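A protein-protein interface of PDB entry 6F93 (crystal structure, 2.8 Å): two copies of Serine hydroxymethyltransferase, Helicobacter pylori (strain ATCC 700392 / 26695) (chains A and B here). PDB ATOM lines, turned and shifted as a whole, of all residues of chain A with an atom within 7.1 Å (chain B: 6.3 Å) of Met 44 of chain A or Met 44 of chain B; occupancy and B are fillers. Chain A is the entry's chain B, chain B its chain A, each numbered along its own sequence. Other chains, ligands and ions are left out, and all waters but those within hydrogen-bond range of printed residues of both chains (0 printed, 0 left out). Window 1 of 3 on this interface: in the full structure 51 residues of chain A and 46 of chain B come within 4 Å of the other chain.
The backbone carbonyl oxygen (O) of Ala 43 of chain A is in hydrogen-bond range of the side-chain hydroxyl (OG) of Ser 46 of chain A (2.8 Å).
The backbone NH (N) of Leu 48 of chain A sits close to the side-chain hydroxyl (OG) of Ser 46 of chain A (3.4 Å).
O of Ser 46 of chain A sits at hydrogen-bond distance from OG1 of Thr 49 of chain A, 3.1 Å away.
OG of Ser 46 of chain B lies within hydrogen-bond range of O of Ala 43 of chain B.
Leu 5 of chain A touches Ser 39 of chain B (CD1 to O, 3.7 Å).
Ala 43 of chain B touches Leu 5 of chain A.
CG2 of Ile 16 of chain A touches CB of Ser 46 of chain B, 3.9 Å away.
O of Met 41 of chain A touches CA of Gly 45 of chain B, 3.5 Å away.
Met 41 of chain A touches Ser 46 of chain B (SD to O, 3.9 Å).
Met 44 of chain A touches His 262 of chain B (CE to NE2, 3.3 Å).
O of Ser 46 of chain A touches CG of Met 41 of chain B (3.8 Å).
Arg 232 of chain B touches Thr 49 of chain A (CD to O, 3.9 Å).
CD1 of Leu 260 of chain A touches NH2 of Arg 232 of chain B (3.4 Å).
His 262 of chain A touches Met 44 of chain B (NE2 to CE, 3.4 Å).
Of chain B, only Met 44 (3.7 Å) and His 262 (3.3 Å) come within 4 Å of Met 44 of chain A.
Met 44 of chain B touches just these residues of chain A: Met 44 and His 262.
Of the printed residues of chain B, Ile 415 of chain A touches Glu 42.
Printed residues of chain B within 4 Å of Thr 36 of chain A: Thr 49.
Ala 266 of chain A touches none of the printed residues of chain B.
The nearest residue of chain A that does not touch Met 44 of chain B is Gly 45 of chain A (4.5 Å).
The nearest printed residue of chain B that does not touch Val 47 of chain A is Arg 232 of chain B (8.9 Å).
Of the 14 printed residues of chain B, 10 touch a printed residue of chain A.
Hydrophobic or aromatic side chains of chain B that line the printed part of chain A: Met 41, Met 44 and His 262.
Of the 26 printed residues of chain A, 14 touch a printed residue of chain B.
Hydrophobic or aromatic side chains of chain A within 4 Å of the printed part of chain B: Leu 5, Ile 16, Met 41, Met 44, Val 47, Leu 260, His 262, Ile 415 and Phe 416.
Met 41 of chain A touches Gly 45 of chain B, and with the chains exchanged Gly 45 of chain A touches Met 41 of chain B.
Met 41 of chain A touches Thr 49 of chain B, but with the chains exchanged Thr 49 of chain A does not touch Met 41 of chain B (4.2 Å).
Met 44 of chain A touches His 262 of chain B, and with the chains exchanged His 262 of chain A touches Met 44 of chain B.
Thr 49 of chain A touches Arg 232 of chain B, and with the chains exchanged Arg 232 of chain A touches Thr 49 of chain B.
14 positions are printed for both chains.
The backbone NH of Phe 416 of chain A sits close to the backbone carbonyl oxygen of Gly 45 of chain B (3.4 Å).
The backbone NH (N) of Leu 5 of chain A sits at hydrogen-bond distance from the side-chain carboxylate (OE1) of Glu 42 of chain B (2.9 Å).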
ATOM      1  N   LEU A   5      -6.189 -31.331  -4.613  1.00  0.00           N
ATOM      2  CA  LEU A   5      -6.995 -31.767  -5.749  1.00  0.00           C
ATOM      3  C   LEU A   5      -6.133 -32.355  -6.858  1.00  0.00           C
ATOM      4  O   LEU A   5      -6.543 -33.312  -7.524  1.00  0.00           O
ATOM      5  CB  LEU A   5      -7.837 -30.603  -6.268  1.00  0.00           C
ATOM      6  CG  LEU A   5      -9.224 -30.526  -5.633  1.00  0.00           C
ATOM      7  CD1 LEU A   5      -9.882 -29.184  -5.880  1.00  0.00           C
ATOM      8  CD2 LEU A   5     -10.074 -31.645  -6.181  1.00  0.00           C
ATOM      9  N   ILE A  16     -10.960 -27.448 -13.290  1.00  0.00           N
ATOM     10  CA  ILE A  16     -10.689 -26.166 -12.642  1.00  0.00           C
ATOM     11  C   ILE A  16      -9.592 -25.419 -13.387  1.00  0.00           C
ATOM     12  O   ILE A  16      -9.724 -24.229 -13.696  1.00  0.00           O
ATOM     13  CB  ILE A  16     -10.313 -26.382 -11.166  1.00  0.00           C
ATOM     14  CG1 ILE A  16     -11.520 -26.879 -10.370  1.00  0.00           C
ATOM     15  CG2 ILE A  16      -9.725 -25.108 -10.565  1.00  0.00           C
ATOM     16  CD1 ILE A  16     -11.153 -27.411  -9.004  1.00  0.00           C
ATOM     17  N   THR A  36     -13.917 -12.224  -9.736  1.00  0.00           N
ATOM     18  CA  THR A  36     -13.972 -11.971  -8.302  1.00  0.00           C
ATOM     19  C   THR A  36     -12.572 -11.726  -7.741  1.00  0.00           C
ATOM     20  O   THR A  36     -11.579 -12.257  -8.244  1.00  0.00           O
ATOM     21  CB  THR A  36     -14.630 -13.158  -7.594  1.00  0.00           C
ATOM     22  OG1 THR A  36     -15.859 -13.484  -8.256  1.00  0.00           O
ATOM     23  CG2 THR A  36     -14.930 -12.827  -6.151  1.00  0.00           C
ATOM     24  N   SER A  39      -8.890 -12.421  -2.937  1.00  0.00           N
ATOM     25  CA  SER A  39      -9.130 -12.597  -1.508  1.00  0.00           C
ATOM     26  C   SER A  39     -10.533 -13.132  -1.233  1.00  0.00           C
ATOM     27  O   SER A  39     -10.723 -13.938  -0.314  1.00  0.00           O
ATOM     28  CB  SER A  39      -8.911 -11.275  -0.778  1.00  0.00           C
ATOM     29  OG  SER A  39      -9.471 -10.208  -1.516  1.00  0.00           O
ATOM     30  N   VAL A  40     -11.530 -12.686  -2.006  1.00  0.00           N
ATOM     31  CA  VAL A  40     -12.895 -13.168  -1.801  1.00  0.00           C
ATOM     32  C   VAL A  40     -12.953 -14.682  -1.969  1.00  0.00           C
ATOM     33  O   VAL A  40     -13.595 -15.385  -1.176  1.00  0.00           O
ATOM     34  CB  VAL A  40     -13.872 -12.455  -2.755  1.00  0.00           C
ATOM     35  CG1 VAL A  40     -15.271 -13.007  -2.584  1.00  0.00           C
ATOM     36  CG2 VAL A  40     -13.875 -10.970  -2.508  1.00  0.00           C
ATOM     37  N   MET A  41     -12.280 -15.210  -2.997  1.00  0.00           N
ATOM     38  CA  MET A  41     -12.227 -16.658  -3.178  1.00  0.00           C
ATOM     39  C   MET A  41     -11.488 -17.331  -2.031  1.00  0.00           C
ATOM     40  O   MET A  41     -11.774 -18.488  -1.696  1.00  0.00           O
ATOM     41  CB  MET A  41     -11.558 -17.000  -4.508  1.00  0.00           C
ATOM     42  CG  MET A  41     -12.282 -16.458  -5.731  1.00  0.00           C
ATOM     43  SD  MET A  41     -11.301 -16.650  -7.231  1.00  0.00           S
ATOM     44  CE  MET A  41     -12.392 -15.968  -8.463  1.00  0.00           C
ATOM     45  N   GLU A  42     -10.544 -16.622  -1.414  1.00  0.00           N
ATOM     46  CA  GLU A  42      -9.810 -17.182  -0.289  1.00  0.00           C
ATOM     47  C   GLU A  42     -10.733 -17.415   0.897  1.00  0.00           C
ATOM     48  O   GLU A  42     -10.632 -18.442   1.582  1.00  0.00           O
ATOM     49  CB  GLU A  42      -8.666 -16.244   0.081  1.00  0.00           C
ATOM     50  CG  GLU A  42      -7.494 -16.880   0.786  1.00  0.00           C
ATOM     51  CD  GLU A  42      -6.419 -15.859   1.103  1.00  0.00           C
ATOM     52  OE1 GLU A  42      -6.113 -15.666   2.299  1.00  0.00           O
ATOM     53  OE2 GLU A  42      -5.900 -15.230   0.152  1.00  0.00           O
ATOM     54  N   ALA A  43     -11.656 -16.479   1.145  1.00  0.00           N
ATOM     55  CA  ALA A  43     -12.622 -16.669   2.221  1.00  0.00           C
ATOM     56  C   ALA A  43     -13.662 -17.714   1.856  1.00  0.00           C
ATOM     57  O   ALA A  43     -14.172 -18.410   2.743  1.00  0.00           O
ATOM     58  CB  ALA A  43     -13.303 -15.346   2.566  1.00  0.00           C
ATOM     59  N   MET A  44     -13.988 -17.837   0.562  1.00  0.00           N
ATOM     60  CA  MET A  44     -14.958 -18.837   0.127  1.00  0.00           C
ATOM     61  C   MET A  44     -14.528 -20.240   0.530  1.00  0.00           C
ATOM     62  O   MET A  44     -15.369 -21.078   0.879  1.00  0.00           O
ATOM     63  CB  MET A  44     -15.154 -18.759  -1.387  1.00  0.00           C
ATOM     64  CG  MET A  44     -16.148 -17.707  -1.868  1.00  0.00           C
ATOM     65  SD  MET A  44     -17.847 -18.084  -1.396  1.00  0.00           S
ATOM     66  CE  MET A  44     -18.185 -19.534  -2.381  1.00  0.00           C
ATOM     67  N   GLY A  45     -13.222 -20.514   0.492  1.00  0.00           N
ATOM     68  CA  GLY A  45     -12.710 -21.820   0.859  1.00  0.00           C
ATOM     69  C   GLY A  45     -12.067 -21.859   2.230  1.00  0.00           C
ATOM     70  O   GLY A  45     -10.992 -22.446   2.404  1.00  0.00           O
ATOM     71  N   SER A  46     -12.712 -21.239   3.213  1.00  0.00           N
ATOM     72  CA  SER A  46     -12.243 -21.243   4.590  1.00  0.00           C
ATOM     73  C   SER A  46     -12.985 -22.300   5.402  1.00  0.00           C
ATOM     74  O   SER A  46     -13.978 -22.881   4.962  1.00  0.00           O
ATOM     75  CB  SER A  46     -12.425 -19.863   5.216  1.00  0.00           C
ATOM     76  OG  SER A  46     -13.797 -19.522   5.272  1.00  0.00           O
ATOM     77  N   VAL A  47     -12.492 -22.538   6.619  1.00  0.00           N
ATOM     78  CA  VAL A  47     -13.088 -23.539   7.500  1.00  0.00           C
ATOM     79  C   VAL A  47     -14.410 -23.006   8.028  1.00  0.00           C
ATOM     80  O   VAL A  47     -15.099 -23.677   8.804  1.00  0.00           O
ATOM     81  CB  VAL A  47     -12.149 -23.915   8.659  1.00  0.00           C
ATOM     82  CG1 VAL A  47     -10.915 -24.637   8.131  1.00  0.00           C
ATOM     83  CG2 VAL A  47     -11.766 -22.672   9.458  1.00  0.00           C
ATOM     84  N   LEU A  48     -14.762 -21.785   7.613  1.00  0.00           N
ATOM     85  CA  LEU A  48     -16.066 -21.217   7.925  1.00  0.00           C
ATOM     86  C   LEU A  48     -17.214 -22.084   7.416  1.00  0.00           C
ATOM     87  O   LEU A  48     -18.331 -21.965   7.929  1.00  0.00           O
ATOM     88  CB  LEU A  48     -16.155 -19.811   7.335  1.00  0.00           C
ATOM     89  CG  LEU A  48     -16.071 -18.570   8.234  1.00  0.00           C
ATOM     90  CD1 LEU A  48     -15.607 -18.887   9.638  1.00  0.00           C
ATOM     91  CD2 LEU A  48     -15.179 -17.521   7.596  1.00  0.00           C
ATOM     92  N   THR A  49     -16.968 -22.940   6.416  1.00  0.00           N
ATOM     93  CA  THR A  49     -17.982 -23.900   5.973  1.00  0.00           C
ATOM     94  C   THR A  49     -18.449 -24.790   7.118  1.00  0.00           C
ATOM     95  O   THR A  49     -19.644 -25.089   7.231  1.00  0.00           O
ATOM     96  CB  THR A  49     -17.443 -24.779   4.840  1.00  0.00           C
ATOM     97  OG1 THR A  49     -16.647 -24.001   3.936  1.00  0.00           O
ATOM     98  CG2 THR A  49     -18.586 -25.427   4.085  1.00  0.00           C
ATOM     99  N   PRO A 231     -18.411 -12.070  -4.268  1.00  0.00           N
ATOM    100  CA  PRO A 231     -19.004 -13.390  -4.478  1.00  0.00           C
ATOM    101  C   PRO A 231     -20.429 -13.238  -4.984  1.00  0.00           C
ATOM    102  O   PRO A 231     -20.999 -12.150  -5.002  1.00  0.00           O
ATOM    103  CB  PRO A 231     -18.971 -14.016  -3.083  1.00  0.00           C
ATOM    104  CG  PRO A 231     -19.144 -12.848  -2.172  1.00  0.00           C
ATOM    105  CD  PRO A 231     -18.490 -11.654  -2.856  1.00  0.00           C
ATOM    106  N   ARG A 232     -21.005 -14.358  -5.393  1.00  0.00           N
ATOM    107  CA  ARG A 232     -22.345 -14.334  -5.953  1.00  0.00           C
ATOM    108  C   ARG A 232     -23.378 -14.393  -4.841  1.00  0.00           C
ATOM    109  O   ARG A 232     -23.314 -15.248  -3.950  1.00  0.00           O
ATOM    110  CB  ARG A 232     -22.531 -15.474  -6.947  1.00  0.00           C
ATOM    111  CG  ARG A 232     -21.413 -15.530  -7.976  1.00  0.00           C
ATOM    112  CD  ARG A 232     -21.779 -16.467  -9.080  1.00  0.00           C
ATOM    113  NE  ARG A 232     -23.228 -16.491  -9.226  1.00  0.00           N
ATOM    114  CZ  ARG A 232     -23.864 -16.980 -10.278  1.00  0.00           C
ATOM    115  NH1 ARG A 232     -25.189 -16.954 -10.312  1.00  0.00           N
ATOM    116  NH2 ARG A 232     -23.173 -17.476 -11.294  1.00  0.00           N
ATOM    117  N   LEU A 260     -24.670 -19.264   5.443  1.00  0.00           N
ATOM    118  CA  LEU A 260     -23.417 -19.724   4.848  1.00  0.00           C
ATOM    119  C   LEU A 260     -22.305 -18.778   5.277  1.00  0.00           C
ATOM    120  O   LEU A 260     -22.036 -17.769   4.622  1.00  0.00           O
ATOM    121  CB  LEU A 260     -23.532 -19.786   3.332  1.00  0.00           C
ATOM    122  CG  LEU A 260     -23.924 -21.116   2.690  1.00  0.00           C
ATOM    123  CD1 LEU A 260     -25.061 -21.792   3.442  1.00  0.00           C
ATOM    124  CD2 LEU A 260     -24.292 -20.894   1.225  1.00  0.00           C
ATOM    125  N   HIS A 262     -19.100 -18.917   5.213  1.00  0.00           N
ATOM    126  CA  HIS A 262     -18.029 -18.653   4.259  1.00  0.00           C
ATOM    127  C   HIS A 262     -18.476 -17.682   3.174  1.00  0.00           C
ATOM    128  O   HIS A 262     -17.661 -16.898   2.673  1.00  0.00           O
ATOM    129  CB  HIS A 262     -17.514 -19.960   3.642  1.00  0.00           C
ATOM    130  CG  HIS A 262     -18.543 -20.735   2.875  1.00  0.00           C
ATOM    131  ND1 HIS A 262     -19.531 -21.476   3.487  1.00  0.00           N
ATOM    132  CD2 HIS A 262     -18.707 -20.919   1.542  1.00  0.00           C
ATOM    133  CE1 HIS A 262     -20.270 -22.068   2.565  1.00  0.00           C
ATOM    134  NE2 HIS A 262     -19.791 -21.747   1.377  1.00  0.00           N
ATOM    135  N   VAL A 263     -19.761 -17.693   2.818  1.00  0.00           N
ATOM    136  CA  VAL A 263     -20.232 -16.790   1.774  1.00  0.00           C
ATOM    137  C   VAL A 263     -20.428 -15.382   2.321  1.00  0.00           C
ATOM    138  O   VAL A 263     -20.108 -14.395   1.650  1.00  0.00           O
ATOM    139  CB  VAL A 263     -21.516 -17.333   1.133  1.00  0.00           C
ATOM    140  CG1 VAL A 263     -21.941 -16.433  -0.020  1.00  0.00           C
ATOM    141  CG2 VAL A 263     -21.299 -18.760   0.655  1.00  0.00           C
ATOM    142  N   ILE A 264     -20.948 -15.261   3.544  1.00  0.00           N
ATOM    143  CA  ILE A 264     -21.092 -13.944   4.154  1.00  0.00           C
ATOM    144  C   ILE A 264     -19.724 -13.331   4.431  1.00  0.00           C
ATOM    145  O   ILE A 264     -19.506 -12.131   4.199  1.00  0.00           O
ATOM    146  CB  ILE A 264     -21.959 -14.045   5.423  1.00  0.00           C
ATOM    147  CG1 ILE A 264     -23.409 -14.339   5.029  1.00  0.00           C
ATOM    148  CG2 ILE A 264     -21.876 -12.770   6.247  1.00  0.00           C
ATOM    149  CD1 ILE A 264     -24.351 -14.531   6.197  1.00  0.00           C
ATOM    150  N   ALA A 265     -18.771 -14.142   4.905  1.00  0.00           N
ATOM    151  CA  ALA A 265     -17.410 -13.647   5.096  1.00  0.00           C
ATOM    152  C   ALA A 265     -16.805 -13.189   3.777  1.00  0.00           C
ATOM    153  O   ALA A 265     -16.073 -12.192   3.733  1.00  0.00           O
ATOM    154  CB  ALA A 265     -16.536 -14.720   5.741  1.00  0.00           C
ATOM    155  N   ALA A 266     -17.109 -13.903   2.689  1.00  0.00           N
ATOM    156  CA  ALA A 266     -16.639 -13.481   1.374  1.00  0.00           C
ATOM    157  C   ALA A 266     -17.210 -12.117   0.992  1.00  0.00           C
ATOM    158  O   ALA A 266     -16.486 -11.259   0.467  1.00  0.00           O
ATOM    159  CB  ALA A 266     -17.004 -14.536   0.334  1.00  0.00           C
ATOM    160  N   LYS A 267     -18.501 -11.894   1.261  1.00  0.00           N
ATOM    161  CA  LYS A 267     -19.130 -10.617   0.926  1.00  0.00           C
ATOM    162  C   LYS A 267     -18.472  -9.454   1.655  1.00  0.00           C
ATOM    163  O   LYS A 267     -18.285  -8.378   1.075  1.00  0.00           O
ATOM    164  CB  LYS A 267     -20.621 -10.659   1.257  1.00  0.00           C
ATOM    165  CG  LYS A 267     -21.460 -11.435   0.285  1.00  0.00           C
ATOM    166  CD  LYS A 267     -22.895 -11.456   0.742  1.00  0.00           C
ATOM    167  CE  LYS A 267     -23.754 -12.219  -0.232  1.00  0.00           C
ATOM    168  NZ  LYS A 267     -25.152 -12.292   0.247  1.00  0.00           N
ATOM    169  N   VAL A 269     -15.396  -9.382   2.576  1.00  0.00           N
ATOM    170  CA  VAL A 269     -14.090  -9.213   1.944  1.00  0.00           C
ATOM    171  C   VAL A 269     -14.205  -8.343   0.698  1.00  0.00           C
ATOM    172  O   VAL A 269     -13.383  -7.442   0.470  1.00  0.00           O
ATOM    173  CB  VAL A 269     -13.474 -10.586   1.624  1.00  0.00           C
ATOM    174  CG1 VAL A 269     -12.237 -10.437   0.745  1.00  0.00           C
ATOM    175  CG2 VAL A 269     -13.129 -11.313   2.905  1.00  0.00           C
ATOM    176  N   ILE A 415      -6.442 -21.895  -7.647  1.00  0.00           N
ATOM    177  CA  ILE A 415      -7.140 -22.162  -6.396  1.00  0.00           C
ATOM    178  C   ILE A 415      -6.465 -21.404  -5.254  1.00  0.00           C
ATOM    179  O   ILE A 415      -5.262 -21.117  -5.293  1.00  0.00           O
ATOM    180  CB  ILE A 415      -7.192 -23.679  -6.092  1.00  0.00           C
ATOM    181  CG1 ILE A 415      -7.495 -24.486  -7.350  1.00  0.00           C
ATOM    182  CG2 ILE A 415      -8.215 -23.974  -5.026  1.00  0.00           C
ATOM    183  CD1 ILE A 415      -7.365 -25.987  -7.180  1.00  0.00           C
ATOM    184  N   PHE A 416      -7.253 -21.080  -4.226  1.00  0.00           N
ATOM    185  CA  PHE A 416      -6.766 -20.262  -3.118  1.00  0.00           C
ATOM    186  C   PHE A 416      -7.005 -20.921  -1.757  1.00  0.00           C
ATOM    187  O   PHE A 416      -8.121 -20.907  -1.227  1.00  0.00           O
ATOM    188  CB  PHE A 416      -7.425 -18.879  -3.163  1.00  0.00           C
ATOM    189  CG  PHE A 416      -7.306 -18.194  -4.504  1.00  0.00           C
ATOM    190  CD1 PHE A 416      -6.345 -17.216  -4.716  1.00  0.00           C
ATOM    191  CD2 PHE A 416      -8.164 -18.519  -5.550  1.00  0.00           C
ATOM    192  CE1 PHE A 416      -6.228 -16.587  -5.949  1.00  0.00           C
ATOM    193  CE2 PHE A 416      -8.052 -17.895  -6.783  1.00  0.00           C
ATOM    194  CZ  PHE A 416      -7.084 -16.926  -6.983  1.00  0.00           C
ATOM    195  N   SER B  39     -10.083 -31.199   0.303  1.00  0.00           N
ATOM    196  CA  SER B  39     -10.198 -31.072  -1.149  1.00  0.00           C
ATOM    197  C   SER B  39     -11.461 -30.325  -1.550  1.00  0.00           C
ATOM    198  O   SER B  39     -11.481 -29.653  -2.591  1.00  0.00           O
ATOM    199  CB  SER B  39     -10.181 -32.451  -1.809  1.00  0.00           C
ATOM    200  OG  SER B  39     -10.146 -33.487  -0.842  1.00  0.00           O
ATOM    201  N   VAL B  40     -12.520 -30.432  -0.745  1.00  0.00           N
ATOM    202  CA  VAL B  40     -13.774 -29.766  -1.076  1.00  0.00           C
ATOM    203  C   VAL B  40     -13.628 -28.262  -0.917  1.00  0.00           C
ATOM    204  O   VAL B  40     -14.032 -27.488  -1.793  1.00  0.00           O
ATOM    205  CB  VAL B  40     -14.922 -30.317  -0.214  1.00  0.00           C
ATOM    206  CG1 VAL B  40     -16.156 -29.437  -0.359  1.00  0.00           C
ATOM    207  CG2 VAL B  40     -15.237 -31.751  -0.602  1.00  0.00           C
ATOM    208  N   MET B  41     -13.044 -27.823   0.204  1.00  0.00           N
ATOM    209  CA  MET B  41     -12.794 -26.396   0.380  1.00  0.00           C
ATOM    210  C   MET B  41     -11.923 -25.850  -0.740  1.00  0.00           C
ATOM    211  O   MET B  41     -12.098 -24.699  -1.155  1.00  0.00           O
ATOM    212  CB  MET B  41     -12.149 -26.130   1.742  1.00  0.00           C
ATOM    213  CG  MET B  41     -13.139 -25.959   2.883  1.00  0.00           C
ATOM    214  SD  MET B  41     -12.525 -26.552   4.475  1.00  0.00           S
ATOM    215  CE  MET B  41     -10.814 -26.031   4.418  1.00  0.00           C
ATOM    216  N   GLU B  42     -10.999 -26.665  -1.255  1.00  0.00           N
ATOM    217  CA  GLU B  42     -10.163 -26.233  -2.370  1.00  0.00           C
ATOM    218  C   GLU B  42     -11.018 -25.866  -3.581  1.00  0.00           C
ATOM    219  O   GLU B  42     -10.921 -24.751  -4.102  1.00  0.00           O
ATOM    220  CB  GLU B  42      -9.152 -27.329  -2.712  1.00  0.00           C
ATOM    221  CG  GLU B  42      -7.702 -26.866  -2.733  1.00  0.00           C
ATOM    222  CD  GLU B  42      -6.712 -28.026  -2.704  1.00  0.00           C
ATOM    223  OE1 GLU B  42      -6.357 -28.539  -3.786  1.00  0.00           O
ATOM    224  OE2 GLU B  42      -6.288 -28.427  -1.598  1.00  0.00           O
ATOM    225  N   ALA B  43     -11.895 -26.775  -4.020  1.00  0.00           N
ATOM    226  CA  ALA B  43     -12.797 -26.452  -5.126  1.00  0.00           C
ATOM    227  C   ALA B  43     -13.729 -25.291  -4.774  1.00  0.00           C
ATOM    228  O   ALA B  43     -14.023 -24.442  -5.624  1.00  0.00           O
ATOM    229  CB  ALA B  43     -13.608 -27.687  -5.523  1.00  0.00           C
ATOM    230  N   MET B  44     -14.192 -25.232  -3.523  1.00  0.00           N
ATOM    231  CA  MET B  44     -15.060 -24.139  -3.101  1.00  0.00           C
ATOM    232  C   MET B  44     -14.392 -22.777  -3.281  1.00  0.00           C
ATOM    233  O   MET B  44     -15.081 -21.768  -3.478  1.00  0.00           O
ATOM    234  CB  MET B  44     -15.463 -24.345  -1.643  1.00  0.00           C
ATOM    235  CG  MET B  44     -16.825 -23.784  -1.275  1.00  0.00           C
ATOM    236  SD  MET B  44     -18.183 -24.793  -1.902  1.00  0.00           S
ATOM    237  CE  MET B  44     -19.598 -23.925  -1.220  1.00  0.00           C
ATOM    238  N   GLY B  45     -13.064 -22.720  -3.220  1.00  0.00           N
ATOM    239  CA  GLY B  45     -12.363 -21.462  -3.387  1.00  0.00           C
ATOM    240  C   GLY B  45     -11.618 -21.346  -4.702  1.00  0.00           C
ATOM    241  O   GLY B  45     -10.563 -20.707  -4.764  1.00  0.00           O
ATOM    242  N   SER B  46     -12.156 -21.948  -5.760  1.00  0.00           N
ATOM    243  CA  SER B  46     -11.517 -21.952  -7.066  1.00  0.00           C
ATOM    244  C   SER B  46     -12.095 -20.845  -7.948  1.00  0.00           C
ATOM    245  O   SER B  46     -13.008 -20.112  -7.563  1.00  0.00           O
ATOM    246  CB  SER B  46     -11.675 -23.318  -7.734  1.00  0.00           C
ATOM    247  OG  SER B  46     -13.042 -23.624  -7.946  1.00  0.00           O
ATOM    248  N   THR B  49     -16.076 -19.966  -9.493  1.00  0.00           N
ATOM    249  CA  THR B  49     -17.097 -19.004  -9.107  1.00  0.00           C
ATOM    250  C   THR B  49     -17.324 -17.942 -10.175  1.00  0.00           C
ATOM    251  O   THR B  49     -18.324 -17.218 -10.103  1.00  0.00           O
ATOM    252  CB  THR B  49     -16.719 -18.330  -7.786  1.00  0.00           C
ATOM    253  OG1 THR B  49     -17.852 -17.634  -7.251  1.00  0.00           O
ATOM    254  CG2 THR B  49     -15.616 -17.331  -8.015  1.00  0.00           C
ATOM    255  N   PRO B 231     -19.579 -30.352   0.537  1.00  0.00           N
ATOM    256  CA  PRO B 231     -20.072 -28.987   0.737  1.00  0.00           C
ATOM    257  C   PRO B 231     -21.480 -28.997   1.297  1.00  0.00           C
ATOM    258  O   PRO B 231     -22.069 -30.062   1.528  1.00  0.00           O
ATOM    259  CB  PRO B 231     -20.044 -28.390  -0.669  1.00  0.00           C
ATOM    260  CG  PRO B 231     -20.233 -29.561  -1.560  1.00  0.00           C
ATOM    261  CD  PRO B 231     -19.528 -30.712  -0.890  1.00  0.00           C
ATOM    262  N   ARG B 232     -22.043 -27.816   1.521  1.00  0.00           N
ATOM    263  CA  ARG B 232     -23.404 -27.740   2.025  1.00  0.00           C
ATOM    264  C   ARG B 232     -24.355 -27.583   0.847  1.00  0.00           C
ATOM    265  O   ARG B 232     -24.236 -26.632   0.061  1.00  0.00           O
ATOM    266  CB  ARG B 232     -23.577 -26.617   3.043  1.00  0.00           C
ATOM    267  CG  ARG B 232     -22.397 -26.486   3.991  1.00  0.00           C
ATOM    268  CD  ARG B 232     -22.855 -26.313   5.450  1.00  0.00           C
ATOM    269  NE  ARG B 232     -23.340 -24.987   5.738  1.00  0.00           N
ATOM    270  CZ  ARG B 232     -24.571 -24.735   6.176  1.00  0.00           C
ATOM    271  NH1 ARG B 232     -25.440 -25.724   6.356  1.00  0.00           N
ATOM    272  NH2 ARG B 232     -24.950 -23.479   6.425  1.00  0.00           N
ATOM    273  N   HIS B 262     -18.603 -23.755  -8.701  1.00  0.00           N
ATOM    274  CA  HIS B 262     -17.648 -24.120  -7.662  1.00  0.00           C
ATOM    275  C   HIS B 262     -18.299 -25.004  -6.607  1.00  0.00           C
ATOM    276  O   HIS B 262     -17.665 -25.926  -6.080  1.00  0.00           O
ATOM    277  CB  HIS B 262     -17.053 -22.863  -7.027  1.00  0.00           C
ATOM    278  CG  HIS B 262     -18.074 -21.921  -6.462  1.00  0.00           C
ATOM    279  ND1 HIS B 262     -18.877 -21.128  -7.254  1.00  0.00           N
ATOM    280  CD2 HIS B 262     -18.405 -21.629  -5.181  1.00  0.00           C
ATOM    281  CE1 HIS B 262     -19.667 -20.398  -6.486  1.00  0.00           C
ATOM    282  NE2 HIS B 262     -19.401 -20.684  -5.224  1.00  0.00           N
ATOM    283  N   VAL B 263     -19.570 -24.752  -6.300  1.00  0.00           N
ATOM    284  CA  VAL B 263     -20.272 -25.594  -5.337  1.00  0.00           C
ATOM    285  C   VAL B 263     -20.547 -26.972  -5.928  1.00  0.00           C
ATOM    286  O   VAL B 263     -20.464 -27.991  -5.227  1.00  0.00           O
ATOM    287  CB  VAL B 263     -21.569 -24.902  -4.878  1.00  0.00           C
ATOM    288  CG1 VAL B 263     -22.222 -25.677  -3.744  1.00  0.00           C
ATOM    289  CG2 VAL B 263     -21.276 -23.478  -4.461  1.00  0.00           C
ATOM    290  N   ALA B 266     -17.374 -28.824  -6.085  1.00  0.00           N
ATOM    291  CA  ALA B 266     -17.144 -29.285  -4.721  1.00  0.00           C
ATOM    292  C   ALA B 266     -17.985 -30.516  -4.419  1.00  0.00           C
ATOM    293  O   ALA B 266     -17.538 -31.422  -3.706  1.00  0.00           O
ATOM    294  CB  ALA B 266     -17.447 -28.167  -3.726  1.00  0.00           C
